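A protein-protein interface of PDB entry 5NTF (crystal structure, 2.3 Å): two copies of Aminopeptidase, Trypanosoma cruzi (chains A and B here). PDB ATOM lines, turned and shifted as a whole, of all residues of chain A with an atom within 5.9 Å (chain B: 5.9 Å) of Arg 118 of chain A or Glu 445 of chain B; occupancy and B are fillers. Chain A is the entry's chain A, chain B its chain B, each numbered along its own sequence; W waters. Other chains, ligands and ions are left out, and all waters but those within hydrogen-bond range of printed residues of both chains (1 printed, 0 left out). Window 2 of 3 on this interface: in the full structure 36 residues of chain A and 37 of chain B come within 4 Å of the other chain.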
ATOM      1  N   VAL A 106      -9.027   2.517  -9.106  1.00  0.00           N
ATOM      2  CA  VAL A 106      -9.922   2.834  -8.003  1.00  0.00           C
ATOM      3  C   VAL A 106     -10.174   4.333  -8.003  1.00  0.00           C
ATOM      4  O   VAL A 106      -9.247   5.082  -8.204  1.00  0.00           O
ATOM      5  CB  VAL A 106      -9.273   2.461  -6.656  1.00  0.00           C
ATOM      6  CG1 VAL A 106     -10.225   2.721  -5.499  1.00  0.00           C
ATOM      7  CG2 VAL A 106      -8.809   1.004  -6.651  1.00  0.00           C
ATOM      8  N   PRO A 107     -11.419   4.784  -7.736  1.00  0.00           N
ATOM      9  CA  PRO A 107     -11.596   6.226  -7.630  1.00  0.00           C
ATOM     10  C   PRO A 107     -10.889   6.762  -6.405  1.00  0.00           C
ATOM     11  O   PRO A 107     -10.738   6.052  -5.415  1.00  0.00           O
ATOM     12  CB  PRO A 107     -13.121   6.397  -7.524  1.00  0.00           C
ATOM     13  CG  PRO A 107     -13.618   5.090  -6.994  1.00  0.00           C
ATOM     14  CD  PRO A 107     -12.689   4.049  -7.533  1.00  0.00           C
ATOM     15  N   SER A 108     -10.433   8.002  -6.478  1.00  0.00           N
ATOM     16  CA  SER A 108      -9.839   8.657  -5.310  1.00  0.00           C
ATOM     17  C   SER A 108     -10.897   9.389  -4.441  1.00  0.00           C
ATOM     18  O   SER A 108     -10.675   9.574  -3.236  1.00  0.00           O
ATOM     19  CB  SER A 108      -8.739   9.628  -5.729  1.00  0.00           C
ATOM     20  OG  SER A 108      -9.236  10.603  -6.624  1.00  0.00           O
ATOM     21  N   GLU A 109     -12.016   9.792  -5.066  1.00  0.00           N
ATOM     22  CA  GLU A 109     -13.077  10.545  -4.375  1.00  0.00           C
ATOM     23  C   GLU A 109     -13.705   9.707  -3.267  1.00  0.00           C
ATOM     24  O   GLU A 109     -14.106   8.554  -3.502  1.00  0.00           O
ATOM     25  CB  GLU A 109     -14.190  11.014  -5.350  1.00  0.00           C
ATOM     26  N   ALA A 110     -13.764  10.290  -2.077  1.00  0.00           N
ATOM     27  CA  ALA A 110     -14.432   9.676  -0.939  1.00  0.00           C
ATOM     28  C   ALA A 110     -15.030  10.730  -0.014  1.00  0.00           C
ATOM     29  O   ALA A 110     -14.355  11.642   0.422  1.00  0.00           O
ATOM     30  CB  ALA A 110     -13.492   8.764  -0.162  1.00  0.00           C
ATOM     31  N   SER A 111     -16.313  10.585   0.279  1.00  0.00           N
ATOM     32  CA  SER A 111     -16.983  11.490   1.193  1.00  0.00           C
ATOM     33  C   SER A 111     -16.481  11.307   2.606  1.00  0.00           C
ATOM     34  O   SER A 111     -15.919  10.257   2.943  1.00  0.00           O
ATOM     35  CB  SER A 111     -18.490  11.226   1.167  1.00  0.00           C
ATOM     36  OG  SER A 111     -18.999  11.782  -0.030  1.00  0.00           O
ATOM     37  N   THR A 113     -18.169  10.475   5.067  1.00  0.00           N
ATOM     38  CA  THR A 113     -18.840   9.326   5.686  1.00  0.00           C
ATOM     39  C   THR A 113     -18.344   8.006   5.149  1.00  0.00           C
ATOM     40  O   THR A 113     -18.894   6.975   5.491  1.00  0.00           O
ATOM     41  CB  THR A 113     -20.358   9.343   5.400  1.00  0.00           C
ATOM     42  OG1 THR A 113     -20.581   9.153   3.990  1.00  0.00           O
ATOM     43  CG2 THR A 113     -20.974  10.675   5.822  1.00  0.00           C
ATOM     44  N   ASN A 114     -17.323   8.045   4.295  1.00  0.00           N
ATOM     45  CA  ASN A 114     -16.840   6.859   3.587  1.00  0.00           C
ATOM     46  C   ASN A 114     -15.367   6.564   3.925  1.00  0.00           C
ATOM     47  O   ASN A 114     -14.654   7.446   4.402  1.00  0.00           O
ATOM     48  CB  ASN A 114     -17.021   7.035   2.070  1.00  0.00           C
ATOM     49  CG  ASN A 114     -17.166   5.709   1.328  1.00  0.00           C
ATOM     50  OD1 ASN A 114     -16.957   4.645   1.888  1.00  0.00           O
ATOM     51  ND2 ASN A 114     -17.514   5.776   0.056  1.00  0.00           N
ATOM     52  N   CYS A 115     -14.940   5.315   3.683  1.00  0.00           N
ATOM     53  CA  CYS A 115     -13.540   4.918   3.791  1.00  0.00           C
ATOM     54  C   CYS A 115     -12.725   5.525   2.629  1.00  0.00           C
ATOM     55  O   CYS A 115     -13.021   5.256   1.464  1.00  0.00           O
ATOM     56  CB  CYS A 115     -13.412   3.409   3.780  1.00  0.00           C
ATOM     57  SG  CYS A 115     -11.695   2.849   3.754  1.00  0.00           S
ATOM     58  N   PRO A 116     -11.696   6.365   2.928  1.00  0.00           N
ATOM     59  CA  PRO A 116     -10.949   7.029   1.820  1.00  0.00           C
ATOM     60  C   PRO A 116     -10.298   6.078   0.809  1.00  0.00           C
ATOM     61  O   PRO A 116     -10.165   6.421  -0.364  1.00  0.00           O
ATOM     62  CB  PRO A 116      -9.850   7.838   2.542  1.00  0.00           C
ATOM     63  CG  PRO A 116     -10.316   7.982   3.955  1.00  0.00           C
ATOM     64  CD  PRO A 116     -11.168   6.766   4.255  1.00  0.00           C
ATOM     65  N   ALA A 117      -9.930   4.886   1.264  1.00  0.00           N
ATOM     66  CA  ALA A 117      -9.352   3.889   0.348  1.00  0.00           C
ATOM     67  C   ALA A 117     -10.379   3.182  -0.599  1.00  0.00           C
ATOM     68  O   ALA A 117      -9.984   2.360  -1.425  1.00  0.00           O
ATOM     69  CB  ALA A 117      -8.547   2.857   1.142  1.00  0.00           C
ATOM     70  N   ARG A 118     -11.670   3.490  -0.458  1.00  0.00           N
ATOM     71  CA  ARG A 118     -12.731   2.995  -1.344  1.00  0.00           C
ATOM     72  C   ARG A 118     -12.654   1.477  -1.550  1.00  0.00           C
ATOM     73  O   ARG A 118     -12.721   0.987  -2.673  1.00  0.00           O
ATOM     74  CB  ARG A 118     -12.697   3.740  -2.667  1.00  0.00           C
ATOM     75  CG  ARG A 118     -13.022   5.214  -2.573  1.00  0.00           C
ATOM     76  CD  ARG A 118     -14.439   5.487  -2.039  1.00  0.00           C
ATOM     77  NE  ARG A 118     -15.474   4.792  -2.802  1.00  0.00           N
ATOM     78  CZ  ARG A 118     -15.993   5.215  -3.948  1.00  0.00           C
ATOM     79  NH1 ARG A 118     -16.920   4.505  -4.559  1.00  0.00           N
ATOM     80  NH2 ARG A 118     -15.598   6.347  -4.497  1.00  0.00           N
ATOM     81  N   PRO A 119     -12.559   0.717  -0.450  1.00  0.00           N
ATOM     82  CA  PRO A 119     -12.608  -0.734  -0.580  1.00  0.00           C
ATOM     83  C   PRO A 119     -13.855  -1.284  -1.250  1.00  0.00           C
ATOM     84  O   PRO A 119     -13.824  -2.416  -1.714  1.00  0.00           O
ATOM     85  CB  PRO A 119     -12.548  -1.230   0.873  1.00  0.00           C
ATOM     86  CG  PRO A 119     -13.058  -0.102   1.694  1.00  0.00           C
ATOM     87  CD  PRO A 119     -12.688   1.147   0.952  1.00  0.00           C
ATOM     88  N   ASP A 120     -14.937  -0.516  -1.299  1.00  0.00           N
ATOM     89  CA  ASP A 120     -16.124  -0.934  -2.075  1.00  0.00           C
ATOM     90  C   ASP A 120     -15.761  -1.300  -3.550  1.00  0.00           C
ATOM     91  O   ASP A 120     -16.193  -2.322  -4.073  1.00  0.00           O
ATOM     92  CB  ASP A 120     -17.231   0.131  -2.029  1.00  0.00           C
ATOM     93  CG  ASP A 120     -16.767   1.512  -2.522  1.00  0.00           C
ATOM     94  OD1 ASP A 120     -15.772   2.059  -1.989  1.00  0.00           O
ATOM     95  OD2 ASP A 120     -17.393   2.050  -3.458  1.00  0.00           O
ATOM     96  N   VAL A 121     -14.923  -0.473  -4.170  1.00  0.00           N
ATOM     97  CA  VAL A 121     -14.487  -0.682  -5.556  1.00  0.00           C
ATOM     98  C   VAL A 121     -13.366  -1.700  -5.665  1.00  0.00           C
ATOM     99  O   VAL A 121     -13.353  -2.521  -6.580  1.00  0.00           O
ATOM    100  CB  VAL A 121     -14.045   0.640  -6.206  1.00  0.00           C
ATOM    101  CG1 VAL A 121     -13.459   0.412  -7.589  1.00  0.00           C
ATOM    102  CG2 VAL A 121     -15.252   1.560  -6.325  1.00  0.00           C
ATOM    103  N   VAL A 122     -12.405  -1.613  -4.758  1.00  0.00           N
ATOM    104  CA  VAL A 122     -11.342  -2.634  -4.625  1.00  0.00           C
ATOM    105  C   VAL A 122     -11.974  -4.036  -4.623  1.00  0.00           C
ATOM    106  O   VAL A 122     -11.598  -4.909  -5.403  1.00  0.00           O
ATOM    107  CB  VAL A 122     -10.531  -2.463  -3.325  1.00  0.00           C
ATOM    108  CG1 VAL A 122      -9.549  -3.605  -3.128  1.00  0.00           C
ATOM    109  CG2 VAL A 122      -9.764  -1.163  -3.329  1.00  0.00           C
ATOM    110  N   ALA A 123     -12.945  -4.223  -3.734  1.00  0.00           N
ATOM    111  CA  ALA A 123     -13.700  -5.489  -3.675  1.00  0.00           C
ATOM    112  C   ALA A 123     -14.314  -5.898  -5.000  1.00  0.00           C
ATOM    113  O   ALA A 123     -14.144  -7.025  -5.442  1.00  0.00           O
ATOM    114  CB  ALA A 123     -14.792  -5.437  -2.629  1.00  0.00           C
ATOM    115  N   CYS B 443     -23.083  11.048   1.070  1.00  0.00           N
ATOM    116  CA  CYS B 443     -22.177  10.117   0.362  1.00  0.00           C
ATOM    117  C   CYS B 443     -22.514  10.097  -1.122  1.00  0.00           C
ATOM    118  O   CYS B 443     -22.985   9.083  -1.641  1.00  0.00           O
ATOM    119  CB  CYS B 443     -22.241   8.709   0.961  1.00  0.00           C
ATOM    120  SG  CYS B 443     -20.874   7.624   0.444  1.00  0.00           S
ATOM    121  N   PRO B 444     -22.307  11.234  -1.819  1.00  0.00           N
ATOM    122  CA  PRO B 444     -22.594  11.399  -3.266  1.00  0.00           C
ATOM    123  C   PRO B 444     -22.149  10.253  -4.140  1.00  0.00           C
ATOM    124  O   PRO B 444     -22.831   9.939  -5.114  1.00  0.00           O
ATOM    125  CB  PRO B 444     -21.767  12.632  -3.645  1.00  0.00           C
ATOM    126  CG  PRO B 444     -21.705  13.429  -2.395  1.00  0.00           C
ATOM    127  CD  PRO B 444     -21.663  12.443  -1.267  1.00  0.00           C
ATOM    128  N   GLU B 445     -20.994   9.657  -3.811  1.00  0.00           N
ATOM    129  CA  GLU B 445     -20.444   8.555  -4.653  1.00  0.00           C
ATOM    130  C   GLU B 445     -21.426   7.378  -4.761  1.00  0.00           C
ATOM    131  O   GLU B 445     -21.441   6.702  -5.780  1.00  0.00           O
ATOM    132  CB  GLU B 445     -19.044   8.064  -4.213  1.00  0.00           C
ATOM    133  CG  GLU B 445     -18.946   7.546  -2.772  1.00  0.00           C
ATOM    134  CD  GLU B 445     -18.414   8.593  -1.785  1.00  0.00           C
ATOM    135  OE1 GLU B 445     -18.717   9.809  -1.967  1.00  0.00           O
ATOM    136  OE2 GLU B 445     -17.688   8.215  -0.828  1.00  0.00           O
ATOM    137  N   TYR B 446     -22.208   7.131  -3.706  1.00  0.00           N
ATOM    138  CA  TYR B 446     -23.204   6.058  -3.725  1.00  0.00           C
ATOM    139  C   TYR B 446     -24.542   6.489  -4.280  1.00  0.00           C
ATOM    140  O   TYR B 446     -25.217   5.694  -4.927  1.00  0.00           O
ATOM    141  CB  TYR B 446     -23.396   5.434  -2.331  1.00  0.00           C
ATOM    142  CG  TYR B 446     -22.168   4.730  -1.802  1.00  0.00           C
ATOM    143  CD1 TYR B 446     -21.094   4.405  -2.638  1.00  0.00           C
ATOM    144  CD2 TYR B 446     -22.080   4.370  -0.446  1.00  0.00           C
ATOM    145  CE1 TYR B 446     -19.968   3.771  -2.127  1.00  0.00           C
ATOM    146  CE2 TYR B 446     -20.951   3.732   0.060  1.00  0.00           C
ATOM    147  CZ  TYR B 446     -19.908   3.436  -0.775  1.00  0.00           C
ATOM    148  OH  TYR B 446     -18.771   2.801  -0.303  1.00  0.00           O
ATOM    149  N   HIS B 447     -24.921   7.734  -4.018  1.00  0.00           N
ATOM    150  CA  HIS B 447     -26.208   8.265  -4.426  1.00  0.00           C
ATOM    151  C   HIS B 447     -26.342   8.435  -5.926  1.00  0.00           C
ATOM    152  O   HIS B 447     -27.385   8.162  -6.477  1.00  0.00           O
ATOM    153  CB  HIS B 447     -26.460   9.631  -3.812  1.00  0.00           C
ATOM    154  CG  HIS B 447     -26.222   9.692  -2.349  1.00  0.00           C
ATOM    155  ND1 HIS B 447     -26.533   8.652  -1.505  1.00  0.00           N
ATOM    156  CD2 HIS B 447     -25.744  10.684  -1.567  1.00  0.00           C
ATOM    157  CE1 HIS B 447     -26.234   8.988  -0.263  1.00  0.00           C
ATOM    158  NE2 HIS B 447     -25.750  10.215  -0.274  1.00  0.00           N
ATOM    159  N   VAL B 448     -25.309   8.934  -6.577  1.00  0.00           N
ATOM    160  CA  VAL B 448     -25.395   9.267  -8.030  1.00  0.00           C
ATOM    161  C   VAL B 448     -25.725   8.076  -8.941  1.00  0.00           C
ATOM    162  O   VAL B 448     -26.314   8.253  -9.989  1.00  0.00           O
ATOM    163  CB  VAL B 448     -24.129   9.990  -8.593  1.00  0.00           C
ATOM    164  CG1 VAL B 448     -23.988  11.380  -7.975  1.00  0.00           C
ATOM    165  CG2 VAL B 448     -22.854   9.162  -8.413  1.00  0.00           C
ATOM    166  N   THR B 449     -25.363   6.876  -8.517  1.00  0.00           N
ATOM    167  CA  THR B 449     -25.568   5.656  -9.291  1.00  0.00           C
ATOM    168  C   THR B 449     -27.033   5.246  -9.358  1.00  0.00           C
ATOM    169  O   THR B 449     -27.463   4.553 -10.295  1.00  0.00           O
ATOM    170  CB  THR B 449     -24.757   4.490  -8.695  1.00  0.00           C
ATOM    171  OG1 THR B 449     -25.027   4.389  -7.291  1.00  0.00           O
ATOM    172  CG2 THR B 449     -23.260   4.747  -8.890  1.00  0.00           C
HETATM  173  O   HOH W   1     -18.898   1.800   1.985  1.00  0.00           O
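ND2 of Asn 114 of chain A lies within hydrogen-bond range of OE2 of Glu 445 of chain B, at 2.6 Å. OG of Ser 111 of chain A is in hydrogen-bond range of OE1 of Glu 445 of chain B, at 2.8 Å. The side-chain amide nitrogen (ND2) of Asn 114 of chain A is in hydrogen-bond range of the side-chain hydroxyl (OH) of Tyr 446 of chain B.
The guanidinium group of Arg 118 of chain A lies within salt-bridge range of the side-chain carboxylate of Asp 120 of chain A (2.7 Å). The side-chain carboxylate of Glu 445 of chain B lies close to the side-chain sulfur of Cys 443 of chain B. The backbone carbonyl oxygen (O) of Tyr 446 of chain B lies within hydrogen-bond range of the side-chain hydroxyl (OG1) of Thr 449 of chain B, at 2.7 Å. The backbone carbonyl oxygen (O) of Glu 109 of chain A lies within hydrogen-bond range of the guanidinium group (NH2) of Arg 118 of chain A (2.8 Å). A ring nitrogen (NE2) of His 447 of chain B sits at hydrogen-bond distance from the backbone NH (N) of Cys 443 of chain B (3.1 Å).
Among the printed residues, merely in contact across the chains: Ser 111 of chain A with Pro 444 of chain B (3.0 Å), Asp 120 of chain A with Tyr 446 of chain B (3.3 Å), Thr 113 of chain A with Cys 443 of chain B (3.5 Å), Ala 110 of chain A with Glu 445 of chain B (3.6 Å), Ser 111 of chain A with Cys 443 of chain B (3.6 Å), Asn 114 of chain A with Cys 443 of chain B (3.9 Å), Arg 118 of chain A with Glu 445 of chain B (3.9 Å) and Arg 118 of chain A with Tyr 446 of chain B (3.97 Å).
Arg 118 of chain A touches just these residues of chain B: Glu 445 and Tyr 446. Of chain A, only Ala 110 (3.6 Å), Ser 111 (2.8 Å), Asn 114 (2.6 Å) and Arg 118 (3.9 Å) come within 4 Å of Glu 445 of chain B. Printed residues of chain B within 4 Å of Asn 114 of chain A: Cys 443 (3.9 Å), Glu 445 (2.6 Å) and Tyr 446 (3.2 Å). Of the printed residues of chain B, Ala 110 of chain A touches Glu 445. Val 121 of chain A touches none of the printed residues of chain B. Ala 123 of chain A touches none of the printed residues of chain B. The nearest printed residue of chain B that does not touch Arg 118 of chain A is Cys 443 of chain B (6.9 Å). The nearest residue of chain A that does not touch Glu 445 of chain B is Glu 109 of chain A (4.5 Å).
Printed residues of chain A that touch a printed residue of chain B: Ala 110, Ser 111, Thr 113, Asn 114, Arg 118 and Asp 120. Of the 7 printed residues of chain B, 4 touch a printed residue of chain A. Printed residues of chain B that touch a printed residue of chain A: Cys 443, Pro 444, Glu 445 and Tyr 446. Hydrophobic or aromatic side chains of chain B that line the printed part of chain A: Pro 444 and Tyr 446.
No position is printed for both chains.
Water W1 lies within hydrogen-bond range of the side-chain hydroxyl (OH) of Tyr 446 of chain B (2.5 Å) and the side-chain amide oxygen (OD1) of Asn 114 of chain A (3.4 Å).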
